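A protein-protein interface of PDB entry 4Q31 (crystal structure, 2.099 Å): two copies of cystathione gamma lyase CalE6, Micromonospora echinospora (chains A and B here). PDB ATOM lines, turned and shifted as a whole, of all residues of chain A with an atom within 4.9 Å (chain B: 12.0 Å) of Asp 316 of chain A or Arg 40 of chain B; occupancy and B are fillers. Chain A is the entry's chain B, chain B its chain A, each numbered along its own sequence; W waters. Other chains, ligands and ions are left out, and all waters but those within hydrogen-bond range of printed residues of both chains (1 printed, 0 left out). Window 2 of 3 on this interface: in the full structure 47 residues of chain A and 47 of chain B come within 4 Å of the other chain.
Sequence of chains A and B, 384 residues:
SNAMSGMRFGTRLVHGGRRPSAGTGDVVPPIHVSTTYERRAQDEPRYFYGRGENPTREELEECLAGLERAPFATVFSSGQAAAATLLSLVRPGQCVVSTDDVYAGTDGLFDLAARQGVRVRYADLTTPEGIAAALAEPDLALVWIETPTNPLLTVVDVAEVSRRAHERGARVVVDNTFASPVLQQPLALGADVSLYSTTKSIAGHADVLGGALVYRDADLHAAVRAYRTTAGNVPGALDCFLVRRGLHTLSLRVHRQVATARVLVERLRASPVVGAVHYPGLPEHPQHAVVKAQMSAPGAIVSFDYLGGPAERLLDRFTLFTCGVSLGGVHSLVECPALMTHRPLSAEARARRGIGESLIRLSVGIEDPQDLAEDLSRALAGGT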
ATOM      1  N   GLU A 312      21.999  16.538  15.775  1.00  0.00           N
ATOM      2  CA  GLU A 312      20.962  16.674  14.758  1.00  0.00           C
ATOM      3  C   GLU A 312      20.584  18.138  14.515  1.00  0.00           C
ATOM      4  O   GLU A 312      20.223  18.509  13.404  1.00  0.00           O
ATOM      5  CB  GLU A 312      19.740  15.796  15.075  1.00  0.00           C
ATOM      6  CG  GLU A 312      19.208  15.938  16.485  1.00  0.00           C
ATOM      7  CD  GLU A 312      18.135  17.001  16.580  1.00  0.00           C
ATOM      8  OE1 GLU A 312      17.765  17.555  15.521  1.00  0.00           O
ATOM      9  OE2 GLU A 312      17.661  17.274  17.702  1.00  0.00           O
ATOM     10  N   ARG A 313      20.712  18.976  15.541  1.00  0.00           N
ATOM     11  CA  ARG A 313      20.480  20.412  15.375  1.00  0.00           C
ATOM     12  C   ARG A 313      21.601  21.068  14.582  1.00  0.00           C
ATOM     13  O   ARG A 313      21.355  21.909  13.716  1.00  0.00           O
ATOM     14  CB  ARG A 313      20.326  21.106  16.729  1.00  0.00           C
ATOM     15  CG  ARG A 313      19.015  20.797  17.431  1.00  0.00           C
ATOM     16  CD  ARG A 313      18.955  21.537  18.746  1.00  0.00           C
ATOM     17  NE  ARG A 313      17.862  21.063  19.576  1.00  0.00           N
ATOM     18  CZ  ARG A 313      17.621  21.514  20.798  1.00  0.00           C
ATOM     19  NH1 ARG A 313      16.614  21.016  21.498  1.00  0.00           N
ATOM     20  NH2 ARG A 313      18.403  22.455  21.318  1.00  0.00           N
ATOM     21  N   LEU A 314      22.837  20.686  14.884  1.00  0.00           N
ATOM     22  CA  LEU A 314      23.980  21.220  14.169  1.00  0.00           C
ATOM     23  C   LEU A 314      23.869  20.920  12.674  1.00  0.00           C
ATOM     24  O   LEU A 314      24.140  21.783  11.838  1.00  0.00           O
ATOM     25  CB  LEU A 314      25.281  20.624  14.726  1.00  0.00           C
ATOM     26  CG  LEU A 314      26.551  20.939  13.928  1.00  0.00           C
ATOM     27  CD1 LEU A 314      26.945  22.381  14.171  1.00  0.00           C
ATOM     28  CD2 LEU A 314      27.696  19.984  14.298  1.00  0.00           C
ATOM     29  N   LEU A 315      23.469  19.694  12.340  1.00  0.00           N
ATOM     30  CA  LEU A 315      23.373  19.274  10.943  1.00  0.00           C
ATOM     31  C   LEU A 315      22.467  20.190  10.108  1.00  0.00           C
ATOM     32  O   LEU A 315      22.728  20.428   8.933  1.00  0.00           O
ATOM     33  CB  LEU A 315      22.894  17.821  10.837  1.00  0.00           C
ATOM     34  CG  LEU A 315      23.841  16.722  11.332  1.00  0.00           C
ATOM     35  CD1 LEU A 315      23.198  15.347  11.174  1.00  0.00           C
ATOM     36  CD2 LEU A 315      25.164  16.774  10.585  1.00  0.00           C
ATOM     37  N   ASP A 316      21.421  20.721  10.725  1.00  0.00           N
ATOM     38  CA  ASP A 316      20.484  21.580  10.005  1.00  0.00           C
ATOM     39  C   ASP A 316      21.022  22.986   9.724  1.00  0.00           C
ATOM     40  O   ASP A 316      20.395  23.755   9.012  1.00  0.00           O
ATOM     41  CB  ASP A 316      19.167  21.693  10.776  1.00  0.00           C
ATOM     42  CG  ASP A 316      18.344  20.423  10.704  1.00  0.00           C
ATOM     43  OD1 ASP A 316      18.556  19.637   9.749  1.00  0.00           O
ATOM     44  OD2 ASP A 316      17.495  20.215  11.601  1.00  0.00           O
ATOM     45  N   ARG A 317      22.172  23.322  10.290  1.00  0.00           N
ATOM     46  CA  ARG A 317      22.674  24.694  10.211  1.00  0.00           C
ATOM     47  C   ARG A 317      23.597  24.951   9.032  1.00  0.00           C
ATOM     48  O   ARG A 317      23.876  26.102   8.697  1.00  0.00           O
ATOM     49  CB  ARG A 317      23.396  25.068  11.501  1.00  0.00           C
ATOM     50  CG  ARG A 317      22.479  25.156  12.707  1.00  0.00           C
ATOM     51  CD  ARG A 317      23.327  25.346  13.952  1.00  0.00           C
ATOM     52  NE  ARG A 317      22.579  25.102  15.172  1.00  0.00           N
ATOM     53  CZ  ARG A 317      23.154  24.978  16.363  1.00  0.00           C
ATOM     54  NH1 ARG A 317      22.412  24.779  17.445  1.00  0.00           N
ATOM     55  NH2 ARG A 317      24.476  25.063  16.466  1.00  0.00           N
ATOM     56  N   PHE A 318      24.092  23.892   8.409  1.00  0.00           N
ATOM     57  CA  PHE A 318      24.993  24.079   7.274  1.00  0.00           C
ATOM     58  C   PHE A 318      24.218  24.613   6.086  1.00  0.00           C
ATOM     59  O   PHE A 318      23.094  24.176   5.824  1.00  0.00           O
ATOM     60  CB  PHE A 318      25.679  22.771   6.918  1.00  0.00           C
ATOM     61  CG  PHE A 318      26.638  22.306   7.964  1.00  0.00           C
ATOM     62  CD1 PHE A 318      27.961  22.728   7.941  1.00  0.00           C
ATOM     63  CD2 PHE A 318      26.215  21.476   8.991  1.00  0.00           C
ATOM     64  CE1 PHE A 318      28.855  22.310   8.916  1.00  0.00           C
ATOM     65  CE2 PHE A 318      27.091  21.060   9.966  1.00  0.00           C
ATOM     66  CZ  PHE A 318      28.420  21.474   9.930  1.00  0.00           C
ATOM     67  N   PHE A 321      27.950  22.992   3.159  1.00  0.00           N
ATOM     68  CA  PHE A 321      28.081  21.535   3.298  1.00  0.00           C
ATOM     69  C   PHE A 321      26.706  20.917   3.105  1.00  0.00           C
ATOM     70  O   PHE A 321      25.714  21.475   3.565  1.00  0.00           O
ATOM     71  CB  PHE A 321      28.554  21.157   4.702  1.00  0.00           C
ATOM     72  CG  PHE A 321      30.018  21.332   4.924  1.00  0.00           C
ATOM     73  CD1 PHE A 321      30.530  22.556   5.315  1.00  0.00           C
ATOM     74  CD2 PHE A 321      30.889  20.266   4.759  1.00  0.00           C
ATOM     75  CE1 PHE A 321      31.890  22.716   5.534  1.00  0.00           C
ATOM     76  CE2 PHE A 321      32.241  20.416   4.984  1.00  0.00           C
ATOM     77  CZ  PHE A 321      32.744  21.645   5.376  1.00  0.00           C
ATOM     78  N   THR A 322      26.641  19.772   2.437  1.00  0.00           N
ATOM     79  CA  THR A 322      25.377  19.043   2.286  1.00  0.00           C
ATOM     80  C   THR A 322      25.314  17.920   3.315  1.00  0.00           C
ATOM     81  O   THR A 322      26.291  17.194   3.512  1.00  0.00           O
ATOM     82  CB  THR A 322      25.246  18.438   0.870  1.00  0.00           C
ATOM     83  OG1 THR A 322      25.251  19.496  -0.087  1.00  0.00           O
ATOM     84  CG2 THR A 322      23.957  17.630   0.711  1.00  0.00           C
ATOM     85  N   CYS A 323      24.169  17.776   3.975  1.00  0.00           N
ATOM     86  CA  CYS A 323      23.999  16.685   4.931  1.00  0.00           C
ATOM     87  C   CYS A 323      23.585  15.415   4.207  1.00  0.00           C
ATOM     88  O   CYS A 323      22.459  15.308   3.731  1.00  0.00           O
ATOM     89  CB  CYS A 323      22.949  17.035   5.993  1.00  0.00           C
ATOM     90  SG  CYS A 323      22.851  15.769   7.274  1.00  0.00           S
ATOM     91  N   THR B  36      23.997  10.569  -4.402  1.00  0.00           N
ATOM     92  CA  THR B  36      23.733  10.967  -3.027  1.00  0.00           C
ATOM     93  C   THR B  36      22.590  11.962  -2.868  1.00  0.00           C
ATOM     94  O   THR B  36      22.206  12.653  -3.814  1.00  0.00           O
ATOM     95  CB  THR B  36      25.010  11.426  -2.290  1.00  0.00           C
ATOM     96  OG1 THR B  36      24.748  11.479  -0.879  1.00  0.00           O
ATOM     97  CG2 THR B  36      25.456  12.772  -2.774  1.00  0.00           C
ATOM     98  N   TYR B  37      22.050  12.011  -1.660  1.00  0.00           N
ATOM     99  CA  TYR B  37      20.831  12.761  -1.393  1.00  0.00           C
ATOM    100  C   TYR B  37      20.945  13.599  -0.139  1.00  0.00           C
ATOM    101  O   TYR B  37      21.497  13.155   0.874  1.00  0.00           O
ATOM    102  CB  TYR B  37      19.642  11.813  -1.262  1.00  0.00           C
ATOM    103  CG  TYR B  37      19.437  10.970  -2.484  1.00  0.00           C
ATOM    104  CD1 TYR B  37      18.698  11.446  -3.567  1.00  0.00           C
ATOM    105  CD2 TYR B  37      19.995   9.698  -2.571  1.00  0.00           C
ATOM    106  CE1 TYR B  37      18.516  10.673  -4.706  1.00  0.00           C
ATOM    107  CE2 TYR B  37      19.816   8.916  -3.700  1.00  0.00           C
ATOM    108  CZ  TYR B  37      19.077   9.409  -4.755  1.00  0.00           C
ATOM    109  OH  TYR B  37      18.897   8.632  -5.858  1.00  0.00           O
ATOM    110  N   GLU B  38      20.430  14.821  -0.230  1.00  0.00           N
ATOM    111  CA  GLU B  38      20.308  15.703   0.919  1.00  0.00           C
ATOM    112  C   GLU B  38      19.144  15.210   1.773  1.00  0.00           C
ATOM    113  O   GLU B  38      18.022  15.027   1.282  1.00  0.00           O
ATOM    114  CB  GLU B  38      20.078  17.150   0.460  1.00  0.00           C
ATOM    115  CG  GLU B  38      19.584  18.117   1.545  1.00  0.00           C
ATOM    116  CD  GLU B  38      20.587  18.325   2.686  1.00  0.00           C
ATOM    117  OE1 GLU B  38      21.656  18.940   2.465  1.00  0.00           O
ATOM    118  OE2 GLU B  38      20.297  17.883   3.819  1.00  0.00           O
ATOM    119  N   ARG B  39      19.428  14.985   3.050  1.00  0.00           N
ATOM    120  CA  ARG B  39      18.433  14.522   4.008  1.00  0.00           C
ATOM    121  C   ARG B  39      17.357  15.572   4.289  1.00  0.00           C
ATOM    122  O   ARG B  39      16.163  15.262   4.305  1.00  0.00           O
ATOM    123  CB  ARG B  39      19.123  14.125   5.313  1.00  0.00           C
ATOM    124  CG  ARG B  39      20.201  13.070   5.137  1.00  0.00           C
ATOM    125  CD  ARG B  39      19.630  11.773   4.574  1.00  0.00           C
ATOM    126  NE  ARG B  39      20.405  10.615   5.011  1.00  0.00           N
ATOM    127  CZ  ARG B  39      20.348  10.095   6.238  1.00  0.00           C
ATOM    128  NH1 ARG B  39      21.091   9.037   6.547  1.00  0.00           N
ATOM    129  NH2 ARG B  39      19.552  10.632   7.158  1.00  0.00           N
ATOM    130  N   ARG B  40      17.789  16.814   4.495  1.00  0.00           N
ATOM    131  CA  ARG B  40      16.898  17.903   4.900  1.00  0.00           C
ATOM    132  C   ARG B  40      15.914  18.378   3.816  1.00  0.00           C
ATOM    133  O   ARG B  40      15.055  19.218   4.083  1.00  0.00           O
ATOM    134  CB  ARG B  40      17.729  19.086   5.413  1.00  0.00           C
ATOM    135  CG  ARG B  40      18.730  18.706   6.508  1.00  0.00           C
ATOM    136  CD  ARG B  40      19.787  19.788   6.723  1.00  0.00           C
ATOM    137  NE  ARG B  40      20.656  19.948   5.559  1.00  0.00           N
ATOM    138  CZ  ARG B  40      21.622  20.859   5.453  1.00  0.00           C
ATOM    139  NH1 ARG B  40      21.858  21.711   6.453  1.00  0.00           N
ATOM    140  NH2 ARG B  40      22.356  20.912   4.341  1.00  0.00           N
ATOM    141  N   ALA B  41      16.034  17.835   2.607  1.00  0.00           N
ATOM    142  CA  ALA B  41      15.207  18.266   1.474  1.00  0.00           C
ATOM    143  C   ALA B  41      14.000  17.355   1.236  1.00  0.00           C
ATOM    144  O   ALA B  41      13.242  17.540   0.278  1.00  0.00           O
ATOM    145  CB  ALA B  41      16.054  18.355   0.208  1.00  0.00           C
ATOM    146  N   GLN B  42      13.837  16.361   2.104  1.00  0.00           N
ATOM    147  CA  GLN B  42      12.759  15.393   1.964  1.00  0.00           C
ATOM    148  C   GLN B  42      11.856  15.457   3.184  1.00  0.00           C
ATOM    149  O   GLN B  42      12.340  15.526   4.317  1.00  0.00           O
ATOM    150  CB  GLN B  42      13.327  13.982   1.803  1.00  0.00           C
ATOM    151  CG  GLN B  42      14.470  13.880   0.799  1.00  0.00           C
ATOM    152  CD  GLN B  42      15.050  12.477   0.711  1.00  0.00           C
ATOM    153  OE1 GLN B  42      14.320  11.496   0.553  1.00  0.00           O
ATOM    154  NE2 GLN B  42      16.367  12.376   0.822  1.00  0.00           N
ATOM    155  N   ASP B  43      10.547  15.441   2.946  1.00  0.00           N
ATOM    156  CA  ASP B  43       9.559  15.509   4.020  1.00  0.00           C
ATOM    157  C   ASP B  43       9.808  14.404   5.039  1.00  0.00           C
ATOM    158  O   ASP B  43      10.113  14.670   6.201  1.00  0.00           O
ATOM    159  CB  ASP B  43       8.141  15.412   3.452  1.00  0.00           C
ATOM    160  CG  ASP B  43       7.841  16.512   2.449  1.00  0.00           C
ATOM    161  OD1 ASP B  43       8.695  16.770   1.572  1.00  0.00           O
ATOM    162  OD2 ASP B  43       6.756  17.125   2.544  1.00  0.00           O
ATOM    163  N   GLU B  44       9.682  13.163   4.588  1.00  0.00           N
ATOM    164  CA  GLU B  44      10.128  12.020   5.369  1.00  0.00           C
ATOM    165  C   GLU B  44      11.118  11.252   4.507  1.00  0.00           C
ATOM    166  O   GLU B  44      10.736  10.645   3.512  1.00  0.00           O
ATOM    167  CB  GLU B  44       8.945  11.149   5.790  1.00  0.00           C
ATOM    168  CG  GLU B  44       7.840  11.937   6.488  1.00  0.00           C
ATOM    169  CD  GLU B  44       7.170  11.159   7.604  1.00  0.00           C
ATOM    170  OE1 GLU B  44       7.871  10.386   8.291  1.00  0.00           O
ATOM    171  OE2 GLU B  44       5.944  11.322   7.793  1.00  0.00           O
ATOM    172  N   PRO B  45      12.405  11.307   4.879  1.00  0.00           N
ATOM    173  CA  PRO B  45      13.528  10.836   4.056  1.00  0.00           C
ATOM    174  C   PRO B  45      13.415   9.380   3.622  1.00  0.00           C
ATOM    175  O   PRO B  45      13.351   8.494   4.467  1.00  0.00           O
ATOM    176  CB  PRO B  45      14.738  11.016   4.982  1.00  0.00           C
ATOM    177  CG  PRO B  45      14.332  12.111   5.914  1.00  0.00           C
ATOM    178  CD  PRO B  45      12.865  11.885   6.155  1.00  0.00           C
ATOM    179  N   ARG B  46      13.385   9.144   2.314  1.00  0.00           N
ATOM    180  CA  ARG B  46      13.446   7.782   1.790  1.00  0.00           C
ATOM    181  C   ARG B  46      14.613   7.568   0.818  1.00  0.00           C
ATOM    182  O   ARG B  46      14.939   6.437   0.470  1.00  0.00           O
ATOM    183  CB  ARG B  46      12.118   7.362   1.150  1.00  0.00           C
ATOM    184  CG  ARG B  46      11.308   8.488   0.538  1.00  0.00           C
ATOM    185  CD  ARG B  46      10.104   7.932  -0.216  1.00  0.00           C
ATOM    186  NE  ARG B  46      10.494   6.853  -1.125  1.00  0.00           N
ATOM    187  CZ  ARG B  46       9.764   6.438  -2.158  1.00  0.00           C
ATOM    188  NH1 ARG B  46       8.600   7.018  -2.428  1.00  0.00           N
ATOM    189  NH2 ARG B  46      10.197   5.448  -2.928  1.00  0.00           N
ATOM    190  N   TYR B  47      15.248   8.649   0.378  1.00  0.00           N
ATOM    191  CA  TYR B  47      16.411   8.507  -0.494  1.00  0.00           C
ATOM    192  C   TYR B  47      17.678   8.851   0.277  1.00  0.00           C
ATOM    193  O   TYR B  47      17.811   9.951   0.819  1.00  0.00           O
ATOM    194  CB  TYR B  47      16.246   9.352  -1.764  1.00  0.00           C
ATOM    195  CG  TYR B  47      15.089   8.857  -2.605  1.00  0.00           C
ATOM    196  CD1 TYR B  47      15.275   7.868  -3.560  1.00  0.00           C
ATOM    197  CD2 TYR B  47      13.801   9.351  -2.408  1.00  0.00           C
ATOM    198  CE1 TYR B  47      14.209   7.389  -4.313  1.00  0.00           C
ATOM    199  CE2 TYR B  47      12.733   8.883  -3.154  1.00  0.00           C
ATOM    200  CZ  TYR B  47      12.939   7.904  -4.102  1.00  0.00           C
ATOM    201  OH  TYR B  47      11.879   7.437  -4.845  1.00  0.00           O
ATOM    202  N   PHE B  48      18.591   7.887   0.348  1.00  0.00           N
ATOM    203  CA  PHE B  48      19.811   8.051   1.138  1.00  0.00           C
ATOM    204  C   PHE B  48      21.061   7.905   0.283  1.00  0.00           C
ATOM    205  O   PHE B  48      21.957   8.742   0.343  1.00  0.00           O
ATOM    206  CB  PHE B  48      19.830   7.052   2.291  1.00  0.00           C
ATOM    207  CG  PHE B  48      18.601   7.117   3.143  1.00  0.00           C
ATOM    208  CD1 PHE B  48      18.445   8.133   4.078  1.00  0.00           C
ATOM    209  CD2 PHE B  48      17.582   6.188   2.986  1.00  0.00           C
ATOM    210  CE1 PHE B  48      17.308   8.206   4.864  1.00  0.00           C
ATOM    211  CE2 PHE B  48      16.437   6.254   3.768  1.00  0.00           C
ATOM    212  CZ  PHE B  48      16.301   7.264   4.707  1.00  0.00           C
ATOM    213  N   TYR B  49      21.090   6.862  -0.544  1.00  0.00           N
ATOM    214  CA  TYR B  49      22.287   6.528  -1.297  1.00  0.00           C
ATOM    215  C   TYR B  49      21.905   5.704  -2.518  1.00  0.00           C
ATOM    216  O   TYR B  49      21.056   4.815  -2.440  1.00  0.00           O
ATOM    217  CB  TYR B  49      23.279   5.764  -0.397  1.00  0.00           C
ATOM    218  CG  TYR B  49      24.617   5.443  -1.051  1.00  0.00           C
ATOM    219  CD1 TYR B  49      25.567   6.447  -1.284  1.00  0.00           C
ATOM    220  CD2 TYR B  49      24.941   4.133  -1.414  1.00  0.00           C
ATOM    221  CE1 TYR B  49      26.797   6.152  -1.868  1.00  0.00           C
ATOM    222  CE2 TYR B  49      26.165   3.832  -1.997  1.00  0.00           C
ATOM    223  CZ  TYR B  49      27.088   4.843  -2.223  1.00  0.00           C
ATOM    224  OH  TYR B  49      28.302   4.533  -2.802  1.00  0.00           O
HETATM  225  O   HOH W   1      23.668  23.002   2.169  1.00  0.00           O
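OE1 of Glu 38 of chain B lies within hydrogen-bond range of N of Cys 323 of chain A.
The backbone carbonyl oxygen (O) of Cys 323 of chain A lies within hydrogen-bond range of the backbone NH (N) of Arg 39 of chain B, at 3.1 Å.
The backbone carbonyl oxygen (O) of Leu 315 of chain A lies within hydrogen-bond range of the guanidinium group (NH1) of Arg 40 of chain B, 2.9 Å away.
NH1 of Arg 40 of chain B lies within hydrogen-bond range of O of Phe 318 of chain A (2.8 Å).
The guanidinium group (NH2) of Arg 40 of chain B lies within hydrogen-bond range of the backbone carbonyl oxygen (O) of Phe 321 of chain A.
OE2 of Glu 38 of chain B lies within salt-bridge range of NE of Arg 40 of chain B (2.7 Å).
The backbone carbonyl oxygen of Glu 38 of chain B lies within hydrogen-bond range of the side-chain amide nitrogen of Gln 42 of chain B, 3.2 Å away.
Asp 316 of chain A touches Arg 40 of chain B.
Thr 322 of chain A touches Glu 38 of chain B (CG2 to OE1, 3.2 Å).
Cys 323 of chain A touches Tyr 37 of chain B (O to O, 3.7 Å).
Cys 323 of chain A touches Arg 40 of chain B.
Asp 316 of chain A touches one residue of chain B.
Of chain A, only Leu 315 (2.9 Å), Asp 316 (3.3 Å), Phe 318 (2.8 Å), Phe 321 (3.5 Å) and Cys 323 (3.6 Å) come within 4 Å of Arg 40 of chain B.
No residue of chain B comes within 4 Å of Leu 314 of chain A.
No residue of chain B comes within 4 Å of Arg 317 of chain A.
Of chain B, only Arg 40 comes within 4 Å of Phe 318 of chain A.
Of chain B, only Glu 38 (3.2 Å) comes within 4 Å of Thr 322 of chain A.
Of chain B, only Tyr 37 (3.7 Å), Glu 38 (3.2 Å), Arg 39 (3.1 Å) and Arg 40 (3.6 Å) come within 4 Å of Cys 323 of chain A.
Printed residues of chain B within 4 Å of Phe 321 of chain A: Arg 40.
Of the printed residues of chain A, Glu 38 of chain B touches Thr 322 (3.2 Å) and Cys 323 (3.2 Å).
Asp 43 of chain B touches none of the printed residues of chain A.
The nearest residue of chain B that does not touch Asp 316 of chain A is Glu 38 of chain B (6.4 Å).
Of the 14 printed residues of chain B, 4 touch a printed residue of chain A.
Printed residues of chain B that touch a printed residue of chain A: Tyr 37, Glu 38, Arg 39 and Arg 40.
No position is printed for both chains.
Water W1 bridges the backbone carbonyl oxygen (O) of Phe 321 of chain A (2.9 Å) and the guanidinium group (NH2) of Arg 40 of chain B (3.3 Å).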
